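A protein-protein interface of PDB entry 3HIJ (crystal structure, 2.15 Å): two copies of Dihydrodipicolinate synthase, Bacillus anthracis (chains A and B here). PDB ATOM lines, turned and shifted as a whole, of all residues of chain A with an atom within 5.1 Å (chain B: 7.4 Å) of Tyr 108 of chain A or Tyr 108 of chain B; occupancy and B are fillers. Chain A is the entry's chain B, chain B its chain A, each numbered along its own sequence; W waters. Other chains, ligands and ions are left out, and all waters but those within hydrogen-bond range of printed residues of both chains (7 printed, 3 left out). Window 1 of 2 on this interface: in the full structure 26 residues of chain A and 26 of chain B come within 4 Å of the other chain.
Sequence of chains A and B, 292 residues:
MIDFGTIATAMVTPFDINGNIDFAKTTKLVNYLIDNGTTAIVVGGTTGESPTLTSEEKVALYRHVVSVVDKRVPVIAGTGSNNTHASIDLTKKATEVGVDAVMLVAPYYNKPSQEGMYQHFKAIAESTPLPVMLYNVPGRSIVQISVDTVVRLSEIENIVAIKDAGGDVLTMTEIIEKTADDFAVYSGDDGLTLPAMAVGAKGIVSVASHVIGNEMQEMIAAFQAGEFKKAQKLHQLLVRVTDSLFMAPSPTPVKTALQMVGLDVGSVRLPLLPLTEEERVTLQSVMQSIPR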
ATOM      1  N   SER A  81      11.634  19.939   2.968  1.00  0.00           N
ATOM      2  CA  SER A  81      11.250  18.524   2.784  1.00  0.00           C
ATOM      3  C   SER A  81      12.297  17.648   3.585  1.00  0.00           C
ATOM      4  O   SER A  81      13.016  18.145   4.498  1.00  0.00           O
ATOM      5  CB  SER A  81      11.276  18.161   1.291  1.00  0.00           C
ATOM      6  OG  SER A  81      12.632  18.281   0.800  1.00  0.00           O
ATOM      7  N   ASN A  82      12.381  16.371   3.262  1.00  0.00           N
ATOM      8  CA  ASN A  82      13.399  15.500   3.906  1.00  0.00           C
ATOM      9  C   ASN A  82      14.703  15.449   3.118  1.00  0.00           C
ATOM     10  O   ASN A  82      15.556  14.585   3.348  1.00  0.00           O
ATOM     11  CB  ASN A  82      12.861  14.095   4.178  1.00  0.00           C
ATOM     12  CG  ASN A  82      12.403  13.356   2.922  1.00  0.00           C
ATOM     13  OD1 ASN A  82      12.049  12.142   2.984  1.00  0.00           O
ATOM     14  ND2 ASN A  82      12.401  14.041   1.785  1.00  0.00           N
ATOM     15  N   VAL A 105       9.977  21.703   7.769  1.00  0.00           N
ATOM     16  CA  VAL A 105       9.457  20.573   8.562  1.00  0.00           C
ATOM     17  C   VAL A 105      10.650  19.688   8.958  1.00  0.00           C
ATOM     18  O   VAL A 105      11.620  19.579   8.203  1.00  0.00           O
ATOM     19  CB  VAL A 105       8.418  19.723   7.691  1.00  0.00           C
ATOM     20  CG1 VAL A 105       9.078  19.096   6.532  1.00  0.00           C
ATOM     21  CG2 VAL A 105       7.667  18.699   8.504  1.00  0.00           C
ATOM     22  N   ALA A 106      10.541  19.035  10.118  1.00  0.00           N
ATOM     23  CA  ALA A 106      11.404  17.940  10.452  1.00  0.00           C
ATOM     24  C   ALA A 106      11.360  16.869   9.353  1.00  0.00           C
ATOM     25  O   ALA A 106      10.286  16.407   8.984  1.00  0.00           O
ATOM     26  CB  ALA A 106      11.057  17.375  11.829  1.00  0.00           C
ATOM     27  N   PRO A 107      12.524  16.454   8.830  1.00  0.00           N
ATOM     28  CA  PRO A 107      12.511  15.403   7.777  1.00  0.00           C
ATOM     29  C   PRO A 107      11.740  14.195   8.181  1.00  0.00           C
ATOM     30  O   PRO A 107      12.050  13.600   9.216  1.00  0.00           O
ATOM     31  CB  PRO A 107      13.991  15.046   7.605  1.00  0.00           C
ATOM     32  CG  PRO A 107      14.663  16.387   7.801  1.00  0.00           C
ATOM     33  CD  PRO A 107      13.867  17.009   9.002  1.00  0.00           C
ATOM     34  N   TYR A 108      10.750  13.853   7.361  1.00  0.00           N
ATOM     35  CA  TYR A 108       9.928  12.649   7.530  1.00  0.00           C
ATOM     36  C   TYR A 108      10.623  11.484   6.813  1.00  0.00           C
ATOM     37  O   TYR A 108      11.521  11.726   5.973  1.00  0.00           O
ATOM     38  CB  TYR A 108       8.521  12.858   6.872  1.00  0.00           C
ATOM     39  CG  TYR A 108       8.637  13.652   5.559  1.00  0.00           C
ATOM     40  CD1 TYR A 108       8.511  15.048   5.550  1.00  0.00           C
ATOM     41  CD2 TYR A 108       8.925  13.002   4.354  1.00  0.00           C
ATOM     42  CE1 TYR A 108       8.679  15.786   4.353  1.00  0.00           C
ATOM     43  CE2 TYR A 108       9.063  13.721   3.123  1.00  0.00           C
ATOM     44  CZ  TYR A 108       8.958  15.127   3.161  1.00  0.00           C
ATOM     45  OH  TYR A 108       9.100  15.851   1.995  1.00  0.00           O
ATOM     46  N   TYR A 109      10.170  10.245   7.095  1.00  0.00           N
ATOM     47  CA  TYR A 109      10.595   9.010   6.385  1.00  0.00           C
ATOM     48  C   TYR A 109      12.053   8.591   6.567  1.00  0.00           C
ATOM     49  O   TYR A 109      12.321   7.444   6.889  1.00  0.00           O
ATOM     50  CB  TYR A 109      10.284   9.138   4.889  1.00  0.00           C
ATOM     51  CG  TYR A 109      10.507   7.862   4.107  1.00  0.00           C
ATOM     52  CD1 TYR A 109       9.686   6.723   4.304  1.00  0.00           C
ATOM     53  CD2 TYR A 109      11.461   7.815   3.111  1.00  0.00           C
ATOM     54  CE1 TYR A 109       9.910   5.561   3.619  1.00  0.00           C
ATOM     55  CE2 TYR A 109      11.645   6.641   2.341  1.00  0.00           C
ATOM     56  CZ  TYR A 109      10.862   5.519   2.610  1.00  0.00           C
ATOM     57  OH  TYR A 109      11.080   4.353   1.857  1.00  0.00           O
ATOM     58  N   ASN A 110      13.024   9.488   6.377  1.00  0.00           N
ATOM     59  CA  ASN A 110      14.404   9.029   6.543  1.00  0.00           C
ATOM     60  C   ASN A 110      14.980   9.103   7.982  1.00  0.00           C
ATOM     61  O   ASN A 110      16.154   8.772   8.198  1.00  0.00           O
ATOM     62  CB  ASN A 110      15.373   9.656   5.549  1.00  0.00           C
ATOM     63  CG  ASN A 110      15.285  11.171   5.476  1.00  0.00           C
ATOM     64  OD1 ASN A 110      14.645  11.803   6.292  1.00  0.00           O
ATOM     65  ND2 ASN A 110      15.973  11.763   4.471  1.00  0.00           N
ATOM     66  N   LYS A 111      14.177   9.564   8.942  1.00  0.00           N
ATOM     67  CA  LYS A 111      14.523   9.488  10.385  1.00  0.00           C
ATOM     68  C   LYS A 111      15.932  10.034  10.741  1.00  0.00           C
ATOM     69  O   LYS A 111      16.777   9.300  11.233  1.00  0.00           O
ATOM     70  CB  LYS A 111      14.315   8.062  10.900  1.00  0.00           C
ATOM     71  CG  LYS A 111      12.822   7.609  10.676  1.00  0.00           C
ATOM     72  CD  LYS A 111      12.470   6.540  11.659  1.00  0.00           C
ATOM     73  CE  LYS A 111      13.285   5.302  11.215  1.00  0.00           C
ATOM     74  NZ  LYS A 111      13.351   4.211  12.236  1.00  0.00           N
ATOM     75  N   ARG A 140       3.764  12.932  12.039  1.00  0.00           N
ATOM     76  CA  ARG A 140       4.019  12.706  10.595  1.00  0.00           C
ATOM     77  C   ARG A 140       5.452  12.383  10.287  1.00  0.00           C
ATOM     78  O   ARG A 140       5.688  11.687   9.343  1.00  0.00           O
ATOM     79  CB  ARG A 140       3.605  13.890   9.698  1.00  0.00           C
ATOM     80  CG  ARG A 140       2.148  14.260   9.828  1.00  0.00           C
ATOM     81  CD  ARG A 140       1.779  15.455   8.905  1.00  0.00           C
ATOM     82  NE  ARG A 140       0.358  15.812   9.127  1.00  0.00           N
ATOM     83  CZ  ARG A 140      -0.657  15.267   8.460  1.00  0.00           C
ATOM     84  NH1 ARG A 140      -0.442  14.370   7.489  1.00  0.00           N
ATOM     85  NH2 ARG A 140      -1.884  15.682   8.686  1.00  0.00           N
ATOM     86  N   SER A 141       6.407  12.918  11.017  1.00  0.00           N
ATOM     87  CA  SER A 141       7.814  12.647  10.686  1.00  0.00           C
ATOM     88  C   SER A 141       8.508  11.595  11.552  1.00  0.00           C
ATOM     89  O   SER A 141       9.669  11.231  11.298  1.00  0.00           O
ATOM     90  CB  SER A 141       8.606  13.942  10.721  1.00  0.00           C
ATOM     91  OG  SER A 141       8.146  14.783   9.631  1.00  0.00           O
ATOM     92  N   SER B  50      16.565   6.901  -1.342  1.00  0.00           N
ATOM     93  CA  SER B  50      15.596   7.441  -2.271  1.00  0.00           C
ATOM     94  C   SER B  50      15.152   8.909  -1.956  1.00  0.00           C
ATOM     95  O   SER B  50      14.911   9.647  -2.869  1.00  0.00           O
ATOM     96  CB  SER B  50      14.358   6.531  -2.383  1.00  0.00           C
ATOM     97  OG  SER B  50      13.651   6.448  -1.142  1.00  0.00           O
ATOM     98  N   PRO B  51      15.043   9.316  -0.680  1.00  0.00           N
ATOM     99  CA  PRO B  51      14.604  10.687  -0.386  1.00  0.00           C
ATOM    100  C   PRO B  51      15.542  11.804  -0.899  1.00  0.00           C
ATOM    101  O   PRO B  51      15.054  12.907  -1.262  1.00  0.00           O
ATOM    102  CB  PRO B  51      14.599  10.718   1.147  1.00  0.00           C
ATOM    103  CG  PRO B  51      14.366   9.280   1.555  1.00  0.00           C
ATOM    104  CD  PRO B  51      15.252   8.556   0.567  1.00  0.00           C
ATOM    105  N   LYS B  58      17.522   8.650 -10.000  1.00  0.00           N
ATOM    106  CA  LYS B  58      16.913   7.339  -9.843  1.00  0.00           C
ATOM    107  C   LYS B  58      16.847   6.604 -11.167  1.00  0.00           C
ATOM    108  O   LYS B  58      17.183   5.451 -11.231  1.00  0.00           O
ATOM    109  CB  LYS B  58      15.533   7.471  -9.260  1.00  0.00           C
ATOM    110  CG  LYS B  58      15.587   8.013  -7.857  1.00  0.00           C
ATOM    111  CD  LYS B  58      14.135   8.219  -7.358  1.00  0.00           C
ATOM    112  CE  LYS B  58      14.136   9.167  -6.111  1.00  0.00           C
ATOM    113  NZ  LYS B  58      12.780   9.184  -5.550  1.00  0.00           N
ATOM    114  N   GLY B  80       7.891   4.006  -5.772  1.00  0.00           N
ATOM    115  CA  GLY B  80       6.752   4.667  -5.091  1.00  0.00           C
ATOM    116  C   GLY B  80       7.181   5.777  -4.150  1.00  0.00           C
ATOM    117  O   GLY B  80       8.240   5.699  -3.524  1.00  0.00           O
ATOM    118  N   SER B  81       6.385   6.840  -4.052  1.00  0.00           N
ATOM    119  CA  SER B  81       6.614   7.843  -3.053  1.00  0.00           C
ATOM    120  C   SER B  81       5.257   8.064  -2.438  1.00  0.00           C
ATOM    121  O   SER B  81       4.365   7.210  -2.534  1.00  0.00           O
ATOM    122  CB  SER B  81       7.147   9.132  -3.692  1.00  0.00           C
ATOM    123  OG  SER B  81       6.289   9.535  -4.743  1.00  0.00           O
ATOM    124  N   ASN B  82       5.106   9.196  -1.775  1.00  0.00           N
ATOM    125  CA  ASN B  82       3.830   9.568  -1.205  1.00  0.00           C
ATOM    126  C   ASN B  82       2.926  10.427  -2.142  1.00  0.00           C
ATOM    127  O   ASN B  82       1.951  11.000  -1.700  1.00  0.00           O
ATOM    128  CB  ASN B  82       4.047  10.239   0.144  1.00  0.00           C
ATOM    129  CG  ASN B  82       4.758  11.582   0.034  1.00  0.00           C
ATOM    130  OD1 ASN B  82       4.924  12.309   1.057  1.00  0.00           O
ATOM    131  ND2 ASN B  82       5.154  11.947  -1.168  1.00  0.00           N
ATOM    132  N   ASN B  83       3.285  10.476  -3.425  1.00  0.00           N
ATOM    133  CA  ASN B  83       2.567  11.222  -4.440  1.00  0.00           C
ATOM    134  C   ASN B  83       2.236  10.179  -5.535  1.00  0.00           C
ATOM    135  O   ASN B  83       3.136   9.639  -6.162  1.00  0.00           O
ATOM    136  CB  ASN B  83       3.545  12.295  -4.980  1.00  0.00           C
ATOM    137  CG  ASN B  83       3.009  13.039  -6.199  1.00  0.00           C
ATOM    138  OD1 ASN B  83       2.114  12.575  -6.867  1.00  0.00           O
ATOM    139  ND2 ASN B  83       3.553  14.232  -6.450  1.00  0.00           N
ATOM    140  N   SER B  87       4.539   8.855  -8.611  1.00  0.00           N
ATOM    141  CA  SER B  87       4.866   7.442  -8.563  1.00  0.00           C
ATOM    142  C   SER B  87       4.540   6.735  -9.850  1.00  0.00           C
ATOM    143  O   SER B  87       5.290   5.849 -10.289  1.00  0.00           O
ATOM    144  CB  SER B  87       4.169   6.766  -7.416  1.00  0.00           C
ATOM    145  OG  SER B  87       4.582   7.318  -6.159  1.00  0.00           O
ATOM    146  N   VAL B 105       6.410   1.883  -1.706  1.00  0.00           N
ATOM    147  CA  VAL B 105       6.226   2.118  -0.252  1.00  0.00           C
ATOM    148  C   VAL B 105       4.868   2.662   0.142  1.00  0.00           C
ATOM    149  O   VAL B 105       4.225   3.402  -0.615  1.00  0.00           O
ATOM    150  CB  VAL B 105       7.350   3.089   0.267  1.00  0.00           C
ATOM    151  CG1 VAL B 105       7.175   4.555  -0.246  1.00  0.00           C
ATOM    152  CG2 VAL B 105       7.431   3.013   1.777  1.00  0.00           C
ATOM    153  N   ALA B 106       4.410   2.361   1.331  1.00  0.00           N
ATOM    154  CA  ALA B 106       3.215   3.059   1.881  1.00  0.00           C
ATOM    155  C   ALA B 106       3.555   4.534   1.956  1.00  0.00           C
ATOM    156  O   ALA B 106       4.641   4.870   2.444  1.00  0.00           O
ATOM    157  CB  ALA B 106       2.903   2.563   3.291  1.00  0.00           C
ATOM    158  N   PRO B 107       2.678   5.421   1.414  1.00  0.00           N
ATOM    159  CA  PRO B 107       2.963   6.866   1.442  1.00  0.00           C
ATOM    160  C   PRO B 107       3.287   7.335   2.864  1.00  0.00           C
ATOM    161  O   PRO B 107       2.504   7.080   3.815  1.00  0.00           O
ATOM    162  CB  PRO B 107       1.656   7.503   0.944  1.00  0.00           C
ATOM    163  CG  PRO B 107       1.241   6.530  -0.109  1.00  0.00           C
ATOM    164  CD  PRO B 107       1.473   5.133   0.610  1.00  0.00           C
ATOM    165  N   TYR B 108       4.446   7.969   3.008  1.00  0.00           N
ATOM    166  CA  TYR B 108       4.849   8.561   4.279  1.00  0.00           C
ATOM    167  C   TYR B 108       4.322  10.005   4.377  1.00  0.00           C
ATOM    168  O   TYR B 108       3.899  10.603   3.362  1.00  0.00           O
ATOM    169  CB  TYR B 108       6.394   8.587   4.322  1.00  0.00           C
ATOM    170  CG  TYR B 108       6.986   8.908   2.941  1.00  0.00           C
ATOM    171  CD1 TYR B 108       7.340   7.872   2.046  1.00  0.00           C
ATOM    172  CD2 TYR B 108       7.179  10.218   2.547  1.00  0.00           C
ATOM    173  CE1 TYR B 108       7.848   8.126   0.789  1.00  0.00           C
ATOM    174  CE2 TYR B 108       7.697  10.517   1.262  1.00  0.00           C
ATOM    175  CZ  TYR B 108       8.040   9.457   0.409  1.00  0.00           C
ATOM    176  OH  TYR B 108       8.524   9.718  -0.822  1.00  0.00           O
ATOM    177  N   TYR B 109       4.402  10.568   5.582  1.00  0.00           N
ATOM    178  CA  TYR B 109       4.113  11.963   5.868  1.00  0.00           C
ATOM    179  C   TYR B 109       2.625  12.421   5.709  1.00  0.00           C
ATOM    180  O   TYR B 109       2.119  13.042   6.617  1.00  0.00           O
ATOM    181  CB  TYR B 109       5.080  12.822   5.074  1.00  0.00           C
ATOM    182  CG  TYR B 109       4.982  14.303   5.365  1.00  0.00           C
ATOM    183  CD1 TYR B 109       5.344  14.819   6.621  1.00  0.00           C
ATOM    184  CD2 TYR B 109       4.601  15.179   4.384  1.00  0.00           C
ATOM    185  CE1 TYR B 109       5.200  16.206   6.906  1.00  0.00           C
ATOM    186  CE2 TYR B 109       4.532  16.577   4.635  1.00  0.00           C
ATOM    187  CZ  TYR B 109       4.841  17.069   5.890  1.00  0.00           C
ATOM    188  OH  TYR B 109       4.782  18.441   6.094  1.00  0.00           O
ATOM    189  N   ASN B 110       1.922  12.099   4.592  1.00  0.00           N
ATOM    190  CA  ASN B 110       0.542  12.551   4.386  1.00  0.00           C
ATOM    191  C   ASN B 110      -0.538  11.660   4.952  1.00  0.00           C
ATOM    192  O   ASN B 110      -1.689  12.003   4.904  1.00  0.00           O
ATOM    193  CB  ASN B 110       0.192  12.970   2.908  1.00  0.00           C
ATOM    194  CG  ASN B 110       0.658  11.973   1.870  1.00  0.00           C
ATOM    195  OD1 ASN B 110       1.017  10.844   2.186  1.00  0.00           O
ATOM    196  ND2 ASN B 110       0.610  12.375   0.580  1.00  0.00           N
ATOM    197  N   LYS B 111      -0.155  10.526   5.478  1.00  0.00           N
ATOM    198  CA  LYS B 111      -1.029   9.677   6.283  1.00  0.00           C
ATOM    199  C   LYS B 111      -2.347   9.320   5.611  1.00  0.00           C
ATOM    200  O   LYS B 111      -3.434   9.575   6.152  1.00  0.00           O
ATOM    201  CB  LYS B 111      -1.213  10.286   7.676  1.00  0.00           C
ATOM    202  CG  LYS B 111       0.107  10.347   8.540  1.00  0.00           C
ATOM    203  CD  LYS B 111      -0.283  10.555  10.030  1.00  0.00           C
ATOM    204  CE  LYS B 111      -1.071  11.883  10.164  1.00  0.00           C
ATOM    205  NZ  LYS B 111      -1.815  12.011  11.515  1.00  0.00           N
ATOM    206  N   PRO B 112      -2.262   8.697   4.420  1.00  0.00           N
ATOM    207  CA  PRO B 112      -3.474   8.260   3.695  1.00  0.00           C
ATOM    208  C   PRO B 112      -4.271   7.240   4.485  1.00  0.00           C
ATOM    209  O   PRO B 112      -3.719   6.609   5.403  1.00  0.00           O
ATOM    210  CB  PRO B 112      -2.928   7.590   2.432  1.00  0.00           C
ATOM    211  CG  PRO B 112      -1.460   7.097   2.826  1.00  0.00           C
ATOM    212  CD  PRO B 112      -1.005   8.197   3.834  1.00  0.00           C
ATOM    213  N   VAL B 137       5.927  -0.108   5.948  1.00  0.00           N
ATOM    214  CA  VAL B 137       6.997   0.336   6.832  1.00  0.00           C
ATOM    215  C   VAL B 137       6.433   1.343   7.844  1.00  0.00           C
ATOM    216  O   VAL B 137       6.744   2.484   7.812  1.00  0.00           O
ATOM    217  CB  VAL B 137       8.276   0.848   6.035  1.00  0.00           C
ATOM    218  CG1 VAL B 137       7.968   2.016   5.091  1.00  0.00           C
ATOM    219  CG2 VAL B 137       9.496   1.132   6.989  1.00  0.00           C
ATOM    220  N   ARG B 140       8.462   4.119   9.430  1.00  0.00           N
ATOM    221  CA  ARG B 140       8.886   5.330   8.690  1.00  0.00           C
ATOM    222  C   ARG B 140       7.720   6.067   8.118  1.00  0.00           C
ATOM    223  O   ARG B 140       7.797   7.288   7.993  1.00  0.00           O
ATOM    224  CB  ARG B 140       9.840   5.029   7.522  1.00  0.00           C
ATOM    225  CG  ARG B 140      11.201   4.423   7.991  1.00  0.00           C
ATOM    226  CD  ARG B 140      12.052   4.076   6.748  1.00  0.00           C
ATOM    227  NE  ARG B 140      13.259   3.455   7.248  1.00  0.00           N
ATOM    228  CZ  ARG B 140      14.337   4.153   7.643  1.00  0.00           C
ATOM    229  NH1 ARG B 140      14.346   5.494   7.573  1.00  0.00           N
ATOM    230  NH2 ARG B 140      15.387   3.513   8.106  1.00  0.00           N
ATOM    231  N   SER B 141       6.653   5.360   7.722  1.00  0.00           N
ATOM    232  CA  SER B 141       5.474   6.047   7.117  1.00  0.00           C
ATOM    233  C   SER B 141       4.339   6.297   8.106  1.00  0.00           C
ATOM    234  O   SER B 141       3.339   6.952   7.776  1.00  0.00           O
ATOM    235  CB  SER B 141       4.930   5.164   5.987  1.00  0.00           C
ATOM    236  OG  SER B 141       5.897   5.193   4.943  1.00  0.00           O
ATOM    237  N   ILE B 142       4.469   5.736   9.299  1.00  0.00           N
ATOM    238  CA  ILE B 142       3.433   5.823  10.361  1.00  0.00           C
ATOM    239  C   ILE B 142       2.206   4.973  10.112  1.00  0.00           C
ATOM    240  O   ILE B 142       1.877   4.167  10.958  1.00  0.00           O
ATOM    241  CB  ILE B 142       3.043   7.283  10.753  1.00  0.00           C
ATOM    242  CG1 ILE B 142       4.308   7.981  11.264  1.00  0.00           C
ATOM    243  CG2 ILE B 142       2.030   7.293  11.976  1.00  0.00           C
ATOM    244  CD1 ILE B 142       4.102   9.393  11.511  1.00  0.00           C
ATOM    245  N   VAL B 143       1.535   5.165   8.974  1.00  0.00           N
ATOM    246  CA  VAL B 143       0.396   4.322   8.651  1.00  0.00           C
ATOM    247  C   VAL B 143       0.956   2.881   8.363  1.00  0.00           C
ATOM    248  O   VAL B 143       2.160   2.693   8.061  1.00  0.00           O
ATOM    249  CB  VAL B 143      -0.357   4.808   7.400  1.00  0.00           C
ATOM    250  CG1 VAL B 143      -1.062   6.230   7.628  1.00  0.00           C
ATOM    251  CG2 VAL B 143       0.616   4.813   6.251  1.00  0.00           C
ATOM    252  N   PRO B 271      19.809  15.002   4.911  1.00  0.00           N
ATOM    253  CA  PRO B 271      20.033  15.235   6.351  1.00  0.00           C
ATOM    254  C   PRO B 271      20.792  14.138   7.101  1.00  0.00           C
ATOM    255  O   PRO B 271      20.911  14.232   8.331  1.00  0.00           O
ATOM    256  CB  PRO B 271      18.594  15.367   6.897  1.00  0.00           C
ATOM    257  CG  PRO B 271      17.817  14.478   5.957  1.00  0.00           C
ATOM    258  CD  PRO B 271      18.405  14.619   4.626  1.00  0.00           C
HETATM  259  O   HOH W   1      11.027  10.856   0.567  1.00  0.00           O
HETATM  260  O   HOH W   2       6.432  14.694   0.900  1.00  0.00           O
HETATM  261  O   HOH W   3      -2.115  14.713   4.806  1.00  0.00           O
HETATM  262  O   HOH W   4      11.648   4.836  -0.733  1.00  0.00           O
HETATM  263  O   HOH W   5      17.107   6.902   6.175  1.00  0.00           O
HETATM  264  O   HOH W   6      12.572  13.762  -0.883  1.00  0.00           O
HETATM  265  O   HOH W   7      14.889   2.345  11.065  1.00  0.00           O
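Water W6 lies within hydrogen-bond range of O of Pro 51 of chain B (2.7 Å) and ND2 of Asn 82 of chain A (2.7 Å). Water W7 bridges NZ of Lys 111 of chain A and NH2 of Arg 140 of chain B. Water W3 lies within hydrogen-bond range of the backbone carbonyl oxygen of Asn 110 of chain B and the guanidinium group of Arg 140 of chain A. Water W2 lies within hydrogen-bond range of the side-chain amide oxygen (OD1) of Asn 82 of chain B (2.8 Å) and the side-chain hydroxyl (OH) of Tyr 108 of chain A (3.1 Å). Water W5 lies within hydrogen-bond range of O of Asn 110 of chain A (2.9 Å) and NH1 of Arg 140 of chain B (3.4 Å). Water W1 bridges OD1 of Asn 82 of chain A and OH of Tyr 108 of chain B.
The backbone carbonyl oxygen (O) of Tyr 109 of chain B sits at hydrogen-bond distance from the guanidinium group (NH1) of Arg 140 of chain A (3.0 Å). O of Tyr 109 of chain A lies within hydrogen-bond range of NH1 of Arg 140 of chain B (2.9 Å).
Among the printed residues, pairs that only touch across the chains: Asn 82 of chain A with Pro 271 of chain B (3.1 Å), Tyr 108 of chain A with Tyr 109 of chain B (3.4 Å), Arg 140 of chain A with Ile 142 of chain B (3.4 Å), Asn 82 of chain A with Pro 51 of chain B (3.5 Å), Tyr 109 of chain A with Tyr 108 of chain B (3.5 Å), Asn 110 of chain A with Pro 271 of chain B (3.6 Å), Tyr 109 of chain A with Pro 51 of chain B (3.6 Å), Asn 110 of chain A with Arg 140 of chain B (3.7 Å), Arg 140 of chain A with Lys 111 of chain B (3.7 Å), Arg 140 of chain A with Asn 110 of chain B (3.7 Å), Asn 110 of chain A with Pro 51 of chain B (3.7 Å), Tyr 108 of chain A with Tyr 108 of chain B (3.8 Å), Val 105 of chain A with Tyr 109 of chain B (3.8 Å), Lys 111 of chain A with Arg 140 of chain B (3.8 Å) and Tyr 109 of chain A with Val 105 of chain B (3.9 Å).
Hydrophobic or aromatic side chains of chain B within 4 Å of the printed part of chain A: Pro 51, Val 105, Tyr 108, Tyr 109, Ile 142 and Pro 271. Of the 11 printed residues of chain A, 7 touch a printed residue of chain B. Among the printed residues, 17 pairs touch across the chains.
Val 105 of chain A touches Tyr 109 of chain B, and with the chains exchanged Tyr 109 of chain A touches Val 105 of chain B. Tyr 108 of chain A touches its own counterpart, Tyr 108 of chain B. Tyr 109 of chain A touches Arg 140 of chain B, and with the chains exchanged Arg 140 of chain A touches Tyr 109 of chain B. Lys 111 of chain A touches Arg 140 of chain B, and with the chains exchanged Arg 140 of chain A touches Lys 111 of chain B. 11 positions are printed for both chains. Of the 17 pairs that touch across the chains among the printed residues, 11 have their exchanged pair printed and touching as well.
Tyr 108 of chain A touches two residues of chain B. Tyr 108 of chain B touches two residues of chain A. Of the printed residues of chain A, Pro 271 of chain B touches Asn 82 and Asn 110. Printed residues of chain A within 4 Å of Pro 51 of chain B: Asn 82, Tyr 109 and Asn 110. Of the printed residues of chain A, Lys 111 of chain B touches Arg 140 (3.7 Å). Of the printed residues of chain B, Asn 110 of chain A touches Pro 51 (3.7 Å), Arg 140 (3.7 Å) and Pro 271 (3.6 Å). Of the printed residues of chain A, Tyr 109 of chain B touches Val 105, Tyr 108 and Arg 140. Ser 141 of chain A touches none of the printed residues of chain B.
The side-chain amide oxygen (OD1) of Asn 82 of chain B sits close to the backbone carbonyl oxygen (O) of Tyr 108 of chain B, 3.0 Å away. The backbone carbonyl oxygen (O) of Asn 82 of chain B sits at hydrogen-bond distance from the side-chain amide nitrogen (ND2) of Asn 110 of chain B, at 3.0 Å. The backbone carbonyl oxygen of Tyr 108 of chain B lies close to the side-chain amide oxygen of Asn 110 of chain B (3.1 Å). OD1 of Asn 82 of chain A sits close to O of Tyr 108 of chain A (3.1 Å). O of Asn 82 of chain A sits at hydrogen-bond distance from ND2 of Asn 110 of chain A, 3.1 Å away. O of Tyr 108 of chain A sits close to OD1 of Asn 110 of chain A, at 3.1 Å.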
